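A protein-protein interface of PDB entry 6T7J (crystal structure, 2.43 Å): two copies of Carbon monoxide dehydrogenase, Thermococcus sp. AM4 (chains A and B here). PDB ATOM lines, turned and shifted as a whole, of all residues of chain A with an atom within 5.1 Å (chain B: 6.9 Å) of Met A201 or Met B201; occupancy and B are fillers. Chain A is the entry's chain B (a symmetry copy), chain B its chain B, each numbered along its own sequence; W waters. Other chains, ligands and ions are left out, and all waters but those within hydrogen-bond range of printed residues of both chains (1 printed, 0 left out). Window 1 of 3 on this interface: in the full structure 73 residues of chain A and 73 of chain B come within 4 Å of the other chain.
Ala A95 touches Met B201, and with the chains exchanged Met A201 touches Ala B95. Ala A98 touches Met B201, and with the chains exchanged Met A201 touches Ala B98. Ala A98 touches His B202, and with the chains exchanged His A202 touches Ala B98. Val A197 touches Cys B198, and with the chains exchanged Cys A198 touches Val B197. 13 positions are printed for both chains. Of the 18 pairs that touch across the chains among the printed residues, 15 have their exchanged pair printed and touching as well.
Water W1 bridges OE2 of Glu B558 (2.5 Å) and NE2 of His A205 (3.3 Å).
Printed residues of chain B that touch a printed residue of chain A: Arg B91, Ala B95, Ala B98, Ala B99, Val B197, Cys B198, Met B201, His B202, His B205 and Glu B558. Of the 13 printed residues of chain A, 8 touch a printed residue of chain B. Hydrophobic or aromatic side chains of chain A within 4 Å of the printed part of chain B: Ala A95, Ala A98, Val A197, Met A201, His A202 and His A205. Along chain A the printed residues that touch a printed residue of chain B span positions 91 to 205.
The side-chain sulfur of Met A201 lies close to the side-chain sulfur of Met B201 (3.5 Å). SG of Cys A198 lies close to O of Ala B98, 3.8 Å away. NH2 of Arg A91 lies within salt-bridge range of OE2 of Glu B558, 3.0 Å away. The backbone carbonyl oxygen (O) of Ala A98 sits close to the side-chain sulfur (SG) of Cys B198 (3.8 Å).
Of chain B, only Ala B95 (3.7 Å), Ala B98 (3.7 Å) and Met B201 (3.5 Å) come within 4 Å of Met A201. Met B201 touches three residues of chain A. Of the printed residues of chain B, Ala A95 touches Arg B91 (3.6 Å), Met B201 (3.7 Å) and His B205 (3.9 Å). Printed residues of chain B within 4 Å of His A205: Ala B95 and Glu B558. Printed residues of chain A within 4 Å of Arg B91: Ala A95. Val B208 touches none of the printed residues of chain A. Ile B206 touches none of the printed residues of chain A. The nearest printed residue of chain B that does not touch His A202 is Ala B95 (4.8 Å).
Arg A91 touches Ala B95 (NH2 to CB, 3.6 Å). CB of Ala A95 touches NH2 of Arg B91 (3.6 Å). CB of Ala A95 touches O of Met B201 (3.7 Å). Ala A95 touches His B205 (O to CD2, 3.9 Å). His B202 touches Ala A98 (N to CB, 3.98 Å). CA of Cys A198 touches CG1 of Val B197, at 3.9 Å. Met A201 touches Ala B95 (O to CB, 3.7 Å). His A202 touches Ala B98. CD2 of His A202 touches CA of Ala B99, at 3.5 Å. His A205 touches Glu B558 (CD2 to OE2, 3.5 Å).
NE of Arg B91 sits at hydrogen-bond distance from OG1 of Thr B204, 2.6 Å away. OG1 of Thr A204 is in hydrogen-bond range of O of Met A201 (3.4 Å). O of Met B201 is in hydrogen-bond range of OG1 of Thr B204, at 3.4 Å. NE of Arg A91 is in hydrogen-bond range of OG1 of Thr A204 (2.6 Å).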
ATOM      1  N   ARG A  91      19.939  14.274  18.891  1.00  0.00           N
ATOM      2  CA  ARG A  91      19.874  12.863  19.262  1.00  0.00           C
ATOM      3  C   ARG A  91      18.705  12.161  18.578  1.00  0.00           C
ATOM      4  O   ARG A  91      18.806  10.973  18.245  1.00  0.00           O
ATOM      5  CB  ARG A  91      19.796  12.713  20.780  1.00  0.00           C
ATOM      6  CG  ARG A  91      21.103  13.068  21.474  1.00  0.00           C
ATOM      7  CD  ARG A  91      21.261  12.367  22.810  1.00  0.00           C
ATOM      8  NE  ARG A  91      22.583  12.620  23.379  1.00  0.00           N
ATOM      9  CZ  ARG A  91      22.926  12.343  24.632  1.00  0.00           C
ATOM     10  NH1 ARG A  91      22.044  11.798  25.458  1.00  0.00           N
ATOM     11  NH2 ARG A  91      24.155  12.613  25.058  1.00  0.00           N
ATOM     12  N   ALA A  94      20.074  11.410  15.223  1.00  0.00           N
ATOM     13  CA  ALA A  94      21.016  10.304  15.355  1.00  0.00           C
ATOM     14  C   ALA A  94      20.292   8.969  15.421  1.00  0.00           C
ATOM     15  O   ALA A  94      20.684   8.011  14.747  1.00  0.00           O
ATOM     16  CB  ALA A  94      21.886  10.502  16.596  1.00  0.00           C
ATOM     17  N   ALA A  95      19.220   8.889  16.215  1.00  0.00           N
ATOM     18  CA  ALA A  95      18.511   7.620  16.364  1.00  0.00           C
ATOM     19  C   ALA A  95      17.810   7.211  15.071  1.00  0.00           C
ATOM     20  O   ALA A  95      17.814   6.028  14.704  1.00  0.00           O
ATOM     21  CB  ALA A  95      17.512   7.710  17.515  1.00  0.00           C
ATOM     22  N   ALA A  98      20.381   6.055  12.661  1.00  0.00           N
ATOM     23  CA  ALA A  98      20.901   4.767  13.108  1.00  0.00           C
ATOM     24  C   ALA A  98      19.953   3.626  12.758  1.00  0.00           C
ATOM     25  O   ALA A  98      20.398   2.549  12.345  1.00  0.00           O
ATOM     26  CB  ALA A  98      21.156   4.802  14.614  1.00  0.00           C
ATOM     27  N   VAL A 197      26.554   9.270  13.191  1.00  0.00           N
ATOM     28  CA  VAL A 197      25.720   8.975  14.358  1.00  0.00           C
ATOM     29  C   VAL A 197      26.529   9.130  15.644  1.00  0.00           C
ATOM     30  O   VAL A 197      26.095   9.780  16.611  1.00  0.00           O
ATOM     31  CB  VAL A 197      25.113   7.564  14.242  1.00  0.00           C
ATOM     32  CG1 VAL A 197      24.630   7.073  15.603  1.00  0.00           C
ATOM     33  CG2 VAL A 197      23.972   7.553  13.234  1.00  0.00           C
ATOM     34  N   CYS A 198      27.728   8.542  15.668  1.00  0.00           N
ATOM     35  CA  CYS A 198      28.550   8.588  16.871  1.00  0.00           C
ATOM     36  C   CYS A 198      28.990  10.013  17.189  1.00  0.00           C
ATOM     37  O   CYS A 198      29.078  10.396  18.361  1.00  0.00           O
ATOM     38  CB  CYS A 198      29.751   7.658  16.702  1.00  0.00           C
ATOM     39  SG  CYS A 198      31.134   7.968  17.803  1.00  0.00           S
ATOM     40  N   GLU A 199      29.243  10.827  16.157  1.00  0.00           N
ATOM     41  CA  GLU A 199      29.618  12.215  16.399  1.00  0.00           C
ATOM     42  C   GLU A 199      28.450  13.018  16.946  1.00  0.00           C
ATOM     43  O   GLU A 199      28.661  13.939  17.741  1.00  0.00           O
ATOM     44  CB  GLU A 199      30.152  12.875  15.125  1.00  0.00           C
ATOM     45  CG  GLU A 199      30.424  14.375  15.297  1.00  0.00           C
ATOM     46  CD  GLU A 199      31.315  14.958  14.219  1.00  0.00           C
ATOM     47  OE1 GLU A 199      31.394  16.202  14.127  1.00  0.00           O
ATOM     48  OE2 GLU A 199      31.938  14.179  13.468  1.00  0.00           O
ATOM     49  N   CYS A 200      27.218  12.710  16.539  1.00  0.00           N
ATOM     50  CA  CYS A 200      26.091  13.369  17.192  1.00  0.00           C
ATOM     51  C   CYS A 200      26.032  12.975  18.665  1.00  0.00           C
ATOM     52  O   CYS A 200      25.870  13.830  19.542  1.00  0.00           O
ATOM     53  CB  CYS A 200      24.767  13.039  16.494  1.00  0.00           C
ATOM     54  SG  CYS A 200      24.553  13.635  14.805  1.00  0.00           S
ATOM     55  N   MET A 201      26.194  11.680  18.954  1.00  0.00           N
ATOM     56  CA  MET A 201      26.184  11.254  20.355  1.00  0.00           C
ATOM     57  C   MET A 201      27.312  11.903  21.155  1.00  0.00           C
ATOM     58  O   MET A 201      27.177  12.104  22.367  1.00  0.00           O
ATOM     59  CB  MET A 201      26.264   9.730  20.451  1.00  0.00           C
ATOM     60  CG  MET A 201      25.012   9.020  19.955  1.00  0.00           C
ATOM     61  SD  MET A 201      23.492   9.839  20.485  1.00  0.00           S
ATOM     62  CE  MET A 201      23.538   9.530  22.253  1.00  0.00           C
ATOM     63  N   HIS A 202      28.423  12.241  20.495  1.00  0.00           N
ATOM     64  CA  HIS A 202      29.521  12.926  21.177  1.00  0.00           C
ATOM     65  C   HIS A 202      29.234  14.415  21.362  1.00  0.00           C
ATOM     66  O   HIS A 202      29.511  14.971  22.430  1.00  0.00           O
ATOM     67  CB  HIS A 202      30.827  12.725  20.401  1.00  0.00           C
ATOM     68  CG  HIS A 202      31.987  13.501  20.949  1.00  0.00           C
ATOM     69  ND1 HIS A 202      32.995  13.994  20.149  1.00  0.00           N
ATOM     70  CD2 HIS A 202      32.301  13.864  22.215  1.00  0.00           C
ATOM     71  CE1 HIS A 202      33.879  14.630  20.897  1.00  0.00           C
ATOM     72  NE2 HIS A 202      33.480  14.568  22.156  1.00  0.00           N
ATOM     73  N   ARG A 203      28.679  15.073  20.340  1.00  0.00           N
ATOM     74  CA  ARG A 203      28.440  16.513  20.409  1.00  0.00           C
ATOM     75  C   ARG A 203      27.433  16.859  21.498  1.00  0.00           C
ATOM     76  O   ARG A 203      27.585  17.868  22.198  1.00  0.00           O
ATOM     77  CB  ARG A 203      27.950  17.030  19.056  1.00  0.00           C
ATOM     78  CG  ARG A 203      29.035  17.226  18.016  1.00  0.00           C
ATOM     79  CD  ARG A 203      28.456  17.794  16.726  1.00  0.00           C
ATOM     80  NE  ARG A 203      29.471  17.933  15.684  1.00  0.00           N
ATOM     81  CZ  ARG A 203      30.068  19.077  15.367  1.00  0.00           C
ATOM     82  NH1 ARG A 203      30.982  19.102  14.407  1.00  0.00           N
ATOM     83  NH2 ARG A 203      29.754  20.194  16.009  1.00  0.00           N
ATOM     84  N   THR A 204      26.395  16.038  21.651  1.00  0.00           N
ATOM     85  CA  THR A 204      25.369  16.264  22.659  1.00  0.00           C
ATOM     86  C   THR A 204      25.815  15.874  24.062  1.00  0.00           C
ATOM     87  O   THR A 204      25.127  16.221  25.030  1.00  0.00           O
ATOM     88  CB  THR A 204      24.103  15.488  22.298  1.00  0.00           C
ATOM     89  OG1 THR A 204      24.388  14.083  22.313  1.00  0.00           O
ATOM     90  CG2 THR A 204      23.618  15.889  20.914  1.00  0.00           C
ATOM     91  N   HIS A 205      26.930  15.155  24.193  1.00  0.00           N
ATOM     92  CA  HIS A 205      27.502  14.868  25.501  1.00  0.00           C
ATOM     93  C   HIS A 205      27.736  16.169  26.260  1.00  0.00           C
ATOM     94  O   HIS A 205      27.957  17.227  25.661  1.00  0.00           O
ATOM     95  CB  HIS A 205      28.813  14.096  25.332  1.00  0.00           C
ATOM     96  CG  HIS A 205      29.375  13.550  26.606  1.00  0.00           C
ATOM     97  ND1 HIS A 205      30.042  14.334  27.523  1.00  0.00           N
ATOM     98  CD2 HIS A 205      29.397  12.290  27.102  1.00  0.00           C
ATOM     99  CE1 HIS A 205      30.435  13.583  28.536  1.00  0.00           C
ATOM    100  NE2 HIS A 205      30.057  12.338  28.305  1.00  0.00           N
ATOM    101  N   LEU B  90      21.117   2.705  28.176  1.00  0.00           N
ATOM    102  CA  LEU B  90      21.829   2.323  26.962  1.00  0.00           C
ATOM    103  C   LEU B  90      22.282   3.551  26.186  1.00  0.00           C
ATOM    104  O   LEU B  90      23.389   3.575  25.637  1.00  0.00           O
ATOM    105  CB  LEU B  90      20.941   1.437  26.088  1.00  0.00           C
ATOM    106  CG  LEU B  90      21.644   0.851  24.866  1.00  0.00           C
ATOM    107  CD1 LEU B  90      22.908   0.183  25.323  1.00  0.00           C
ATOM    108  CD2 LEU B  90      20.764  -0.139  24.121  1.00  0.00           C
ATOM    109  N   ARG B  91      21.442   4.586  26.133  1.00  0.00           N
ATOM    110  CA  ARG B  91      21.846   5.798  25.425  1.00  0.00           C
ATOM    111  C   ARG B  91      22.947   6.540  26.176  1.00  0.00           C
ATOM    112  O   ARG B  91      23.816   7.158  25.547  1.00  0.00           O
ATOM    113  CB  ARG B  91      20.639   6.702  25.183  1.00  0.00           C
ATOM    114  CG  ARG B  91      19.684   6.141  24.140  1.00  0.00           C
ATOM    115  CD  ARG B  91      18.876   7.222  23.448  1.00  0.00           C
ATOM    116  NE  ARG B  91      18.078   6.663  22.360  1.00  0.00           N
ATOM    117  CZ  ARG B  91      17.100   7.312  21.736  1.00  0.00           C
ATOM    118  NH1 ARG B  91      16.795   8.553  22.089  1.00  0.00           N
ATOM    119  NH2 ARG B  91      16.427   6.716  20.759  1.00  0.00           N
ATOM    120  N   MET B  92      22.946   6.472  27.509  1.00  0.00           N
ATOM    121  CA  MET B  92      24.074   7.023  28.263  1.00  0.00           C
ATOM    122  C   MET B  92      25.375   6.310  27.900  1.00  0.00           C
ATOM    123  O   MET B  92      26.413   6.948  27.663  1.00  0.00           O
ATOM    124  CB  MET B  92      23.807   6.919  29.765  1.00  0.00           C
ATOM    125  CG  MET B  92      22.619   7.731  30.251  1.00  0.00           C
ATOM    126  SD  MET B  92      22.527   7.801  32.051  1.00  0.00           S
ATOM    127  CE  MET B  92      23.356   9.360  32.369  1.00  0.00           C
ATOM    128  N   ALA B  94      25.992   4.701  25.151  1.00  0.00           N
ATOM    129  CA  ALA B  94      26.303   5.072  23.775  1.00  0.00           C
ATOM    130  C   ALA B  94      27.022   6.410  23.714  1.00  0.00           C
ATOM    131  O   ALA B  94      28.023   6.550  23.005  1.00  0.00           O
ATOM    132  CB  ALA B  94      25.023   5.115  22.942  1.00  0.00           C
ATOM    133  N   ALA B  95      26.537   7.404  24.466  1.00  0.00           N
ATOM    134  CA  ALA B  95      27.150   8.728  24.412  1.00  0.00           C
ATOM    135  C   ALA B  95      28.557   8.724  25.004  1.00  0.00           C
ATOM    136  O   ALA B  95      29.465   9.372  24.466  1.00  0.00           O
ATOM    137  CB  ALA B  95      26.264   9.744  25.131  1.00  0.00           C
ATOM    138  N   GLY B  96      28.763   8.000  26.107  1.00  0.00           N
ATOM    139  CA  GLY B  96      30.104   7.929  26.677  1.00  0.00           C
ATOM    140  C   GLY B  96      31.092   7.228  25.758  1.00  0.00           C
ATOM    141  O   GLY B  96      32.215   7.710  25.532  1.00  0.00           O
ATOM    142  N   ALA B  98      30.829   7.038  22.608  1.00  0.00           N
ATOM    143  CA  ALA B  98      31.024   7.907  21.451  1.00  0.00           C
ATOM    144  C   ALA B  98      32.031   9.012  21.742  1.00  0.00           C
ATOM    145  O   ALA B  98      32.863   9.341  20.889  1.00  0.00           O
ATOM    146  CB  ALA B  98      29.687   8.506  21.020  1.00  0.00           C
ATOM    147  N   ALA B  99      31.957   9.615  22.930  1.00  0.00           N
ATOM    148  CA  ALA B  99      32.933  10.636  23.293  1.00  0.00           C
ATOM    149  C   ALA B  99      34.347  10.065  23.279  1.00  0.00           C
ATOM    150  O   ALA B  99      35.264  10.636  22.662  1.00  0.00           O
ATOM    151  CB  ALA B  99      32.596  11.218  24.664  1.00  0.00           C
ATOM    152  N   ARG B 195      29.805   1.146  15.019  1.00  0.00           N
ATOM    153  CA  ARG B 195      28.654   0.271  14.833  1.00  0.00           C
ATOM    154  C   ARG B 195      27.965  -0.027  16.159  1.00  0.00           C
ATOM    155  O   ARG B 195      26.736  -0.085  16.222  1.00  0.00           O
ATOM    156  CB  ARG B 195      29.065  -1.031  14.151  1.00  0.00           C
ATOM    157  CG  ARG B 195      27.896  -1.992  13.984  1.00  0.00           C
ATOM    158  CD  ARG B 195      28.335  -3.408  13.686  1.00  0.00           C
ATOM    159  NE  ARG B 195      27.184  -4.276  13.451  1.00  0.00           N
ATOM    160  CZ  ARG B 195      27.258  -5.484  12.905  1.00  0.00           C
ATOM    161  NH1 ARG B 195      26.157  -6.202  12.729  1.00  0.00           N
ATOM    162  NH2 ARG B 195      28.434  -5.976  12.536  1.00  0.00           N
ATOM    163  N   GLU B 196      28.737  -0.221  17.232  1.00  0.00           N
ATOM    164  CA  GLU B 196      28.119  -0.480  18.531  1.00  0.00           C
ATOM    165  C   GLU B 196      27.315   0.725  19.008  1.00  0.00           C
ATOM    166  O   GLU B 196      26.180   0.578  19.487  1.00  0.00           O
ATOM    167  CB  GLU B 196      29.185  -0.861  19.563  1.00  0.00           C
ATOM    168  CG  GLU B 196      30.109  -2.002  19.148  1.00  0.00           C
ATOM    169  CD  GLU B 196      29.367  -3.277  18.787  1.00  0.00           C
ATOM    170  OE1 GLU B 196      28.249  -3.490  19.300  1.00  0.00           O
ATOM    171  OE2 GLU B 196      29.906  -4.075  17.991  1.00  0.00           O
ATOM    172  N   VAL B 197      27.885   1.928  18.872  1.00  0.00           N
ATOM    173  CA  VAL B 197      27.157   3.140  19.255  1.00  0.00           C
ATOM    174  C   VAL B 197      25.869   3.266  18.445  1.00  0.00           C
ATOM    175  O   VAL B 197      24.779   3.510  18.991  1.00  0.00           O
ATOM    176  CB  VAL B 197      28.053   4.382  19.086  1.00  0.00           C
ATOM    177  CG1 VAL B 197      27.208   5.651  19.041  1.00  0.00           C
ATOM    178  CG2 VAL B 197      29.078   4.460  20.208  1.00  0.00           C
ATOM    179  N   CYS B 198      25.975   3.088  17.126  1.00  0.00           N
ATOM    180  CA  CYS B 198      24.811   3.243  16.263  1.00  0.00           C
ATOM    181  C   CYS B 198      23.760   2.176  16.552  1.00  0.00           C
ATOM    182  O   CYS B 198      22.555   2.449  16.488  1.00  0.00           O
ATOM    183  CB  CYS B 198      25.253   3.209  14.800  1.00  0.00           C
ATOM    184  SG  CYS B 198      23.963   2.844  13.607  1.00  0.00           S
ATOM    185  N   GLU B 199      24.193   0.960  16.902  1.00  0.00           N
ATOM    186  CA  GLU B 199      23.234  -0.086  17.239  1.00  0.00           C
ATOM    187  C   GLU B 199      22.529   0.210  18.552  1.00  0.00           C
ATOM    188  O   GLU B 199      21.357  -0.147  18.710  1.00  0.00           O
ATOM    189  CB  GLU B 199      23.912  -1.457  17.311  1.00  0.00           C
ATOM    190  CG  GLU B 199      22.971  -2.564  17.802  1.00  0.00           C
ATOM    191  CD  GLU B 199      23.470  -3.963  17.501  1.00  0.00           C
ATOM    192  OE1 GLU B 199      22.911  -4.925  18.070  1.00  0.00           O
ATOM    193  OE2 GLU B 199      24.415  -4.104  16.696  1.00  0.00           O
ATOM    194  N   CYS B 200      23.205   0.845  19.510  1.00  0.00           N
ATOM    195  CA  CYS B 200      22.476   1.275  20.700  1.00  0.00           C
ATOM    196  C   CYS B 200      21.427   2.319  20.326  1.00  0.00           C
ATOM    197  O   CYS B 200      20.272   2.236  20.756  1.00  0.00           O
ATOM    198  CB  CYS B 200      23.424   1.825  21.770  1.00  0.00           C
ATOM    199  SG  CYS B 200      24.593   0.669  22.511  1.00  0.00           S
ATOM    200  N   MET B 201      21.811   3.294  19.495  1.00  0.00           N
ATOM    201  CA  MET B 201      20.833   4.299  19.075  1.00  0.00           C
ATOM    202  C   MET B 201      19.665   3.674  18.315  1.00  0.00           C
ATOM    203  O   MET B 201      18.549   4.206  18.343  1.00  0.00           O
ATOM    204  CB  MET B 201      21.508   5.380  18.230  1.00  0.00           C
ATOM    205  CG  MET B 201      22.465   6.264  19.018  1.00  0.00           C
ATOM    206  SD  MET B 201      21.816   6.718  20.642  1.00  0.00           S
ATOM    207  CE  MET B 201      20.458   7.796  20.176  1.00  0.00           C
ATOM    208  N   HIS B 202      19.899   2.546  17.639  1.00  0.00           N
ATOM    209  CA  HIS B 202      18.819   1.851  16.941  1.00  0.00           C
ATOM    210  C   HIS B 202      17.951   1.040  17.901  1.00  0.00           C
ATOM    211  O   HIS B 202      16.722   1.043  17.779  1.00  0.00           O
ATOM    212  CB  HIS B 202      19.396   0.947  15.847  1.00  0.00           C
ATOM    213  CG  HIS B 202      18.374   0.090  15.162  1.00  0.00           C
ATOM    214  ND1 HIS B 202      18.665  -1.165  14.673  1.00  0.00           N
ATOM    215  CD2 HIS B 202      17.068   0.309  14.881  1.00  0.00           C
ATOM    216  CE1 HIS B 202      17.582  -1.684  14.122  1.00  0.00           C
ATOM    217  NE2 HIS B 202      16.597  -0.811  14.237  1.00  0.00           N
ATOM    218  N   ARG B 203      18.569   0.345  18.861  1.00  0.00           N
ATOM    219  CA  ARG B 203      17.818  -0.515  19.774  1.00  0.00           C
ATOM    220  C   ARG B 203      16.859   0.293  20.637  1.00  0.00           C
ATOM    221  O   ARG B 203      15.732  -0.144  20.904  1.00  0.00           O
ATOM    222  CB  ARG B 203      18.780  -1.308  20.658  1.00  0.00           C
ATOM    223  CG  ARG B 203      19.414  -2.513  19.992  1.00  0.00           C
ATOM    224  CD  ARG B 203      20.309  -3.267  20.969  1.00  0.00           C
ATOM    225  NE  ARG B 203      20.984  -4.397  20.334  1.00  0.00           N
ATOM    226  CZ  ARG B 203      20.593  -5.662  20.446  1.00  0.00           C
ATOM    227  NH1 ARG B 203      21.269  -6.620  19.828  1.00  0.00           N
ATOM    228  NH2 ARG B 203      19.528  -5.970  21.173  1.00  0.00           N
ATOM    229  N   THR B 204      17.289   1.471  21.088  1.00  0.00           N
ATOM    230  CA  THR B 204      16.460   2.333  21.919  1.00  0.00           C
ATOM    231  C   THR B 204      15.398   3.084  21.128  1.00  0.00           C
ATOM    232  O   THR B 204      14.496   3.671  21.739  1.00  0.00           O
ATOM    233  CB  THR B 204      17.338   3.336  22.666  1.00  0.00           C
ATOM    234  OG1 THR B 204      17.993   4.190  21.718  1.00  0.00           O
ATOM    235  CG2 THR B 204      18.384   2.606  23.493  1.00  0.00           C
ATOM    236  N   HIS B 205      15.492   3.095  19.798  1.00  0.00           N
ATOM    237  CA  HIS B 205      14.440   3.663  18.966  1.00  0.00           C
ATOM    238  C   HIS B 205      13.105   3.008  19.299  1.00  0.00           C
ATOM    239  O   HIS B 205      13.051   1.852  19.733  1.00  0.00           O
ATOM    240  CB  HIS B 205      14.788   3.461  17.488  1.00  0.00           C
ATOM    241  CG  HIS B 205      13.898   4.200  16.539  1.00  0.00           C
ATOM    242  ND1 HIS B 205      12.627   3.771  16.222  1.00  0.00           N
ATOM    243  CD2 HIS B 205      14.107   5.324  15.815  1.00  0.00           C
ATOM    244  CE1 HIS B 205      12.087   4.608  15.356  1.00  0.00           C
ATOM    245  NE2 HIS B 205      12.964   5.559  15.090  1.00  0.00           N
ATOM    246  N   ILE B 206      12.017   3.764  19.123  1.00  0.00           N
ATOM    247  CA  ILE B 206      10.708   3.244  19.497  1.00  0.00           C
ATOM    248  C   ILE B 206      10.419   1.972  18.714  1.00  0.00           C
ATOM    249  O   ILE B 206      10.645   1.898  17.499  1.00  0.00           O
ATOM    250  CB  ILE B 206       9.606   4.294  19.280  1.00  0.00           C
ATOM    251  CG1 ILE B 206       8.252   3.660  19.596  1.00  0.00           C
ATOM    252  CG2 ILE B 206       9.622   4.828  17.848  1.00  0.00           C
ATOM    253  CD1 ILE B 206       7.146   4.626  19.809  1.00  0.00           C
ATOM    254  N   VAL B 208      11.838  -1.116  18.866  1.00  0.00           N
ATOM    255  CA  VAL B 208      12.905  -2.018  18.448  1.00  0.00           C
ATOM    256  C   VAL B 208      13.191  -3.016  19.569  1.00  0.00           C
ATOM    257  O   VAL B 208      12.569  -4.082  19.622  1.00  0.00           O
ATOM    258  CB  VAL B 208      14.160  -1.240  18.012  1.00  0.00           C
ATOM    259  CG1 VAL B 208      15.076  -2.137  17.202  1.00  0.00           C
ATOM    260  CG2 VAL B 208      13.756  -0.040  17.171  1.00  0.00           C
ATOM    261  N   HIS B 218      23.818  -5.534  25.103  1.00  0.00           N
ATOM    262  CA  HIS B 218      24.446  -4.725  24.065  1.00  0.00           C
ATOM    263  C   HIS B 218      25.145  -3.508  24.656  1.00  0.00           C
ATOM    264  O   HIS B 218      26.156  -3.054  24.112  1.00  0.00           O
ATOM    265  CB  HIS B 218      23.434  -4.281  23.015  1.00  0.00           C
ATOM    266  CG  HIS B 218      24.052  -3.491  21.905  1.00  0.00           C
ATOM    267  ND1 HIS B 218      23.819  -2.145  21.728  1.00  0.00           N
ATOM    268  CD2 HIS B 218      24.927  -3.852  20.937  1.00  0.00           C
ATOM    269  CE1 HIS B 218      24.503  -1.719  20.681  1.00  0.00           C
ATOM    270  NE2 HIS B 218      25.191  -2.731  20.190  1.00  0.00           N
ATOM    271  N   GLU B 558      28.176  10.721  30.969  1.00  0.00           N
ATOM    272  CA  GLU B 558      27.866   9.469  30.288  1.00  0.00           C
ATOM    273  C   GLU B 558      29.133   8.664  30.014  1.00  0.00           C
ATOM    274  O   GLU B 558      29.089   7.424  29.962  1.00  0.00           O
ATOM    275  CB  GLU B 558      27.103   9.761  28.993  1.00  0.00           C
ATOM    276  CG  GLU B 558      25.714  10.357  29.218  1.00  0.00           C
ATOM    277  CD  GLU B 558      25.165  11.079  27.995  1.00  0.00           C
ATOM    278  OE1 GLU B 558      24.014  10.795  27.601  1.00  0.00           O
ATOM    279  OE2 GLU B 558      25.881  11.931  27.427  1.00  0.00           O
HETATM  280  O   HOH W   1      27.068  13.328  29.161  1.00  0.00           O
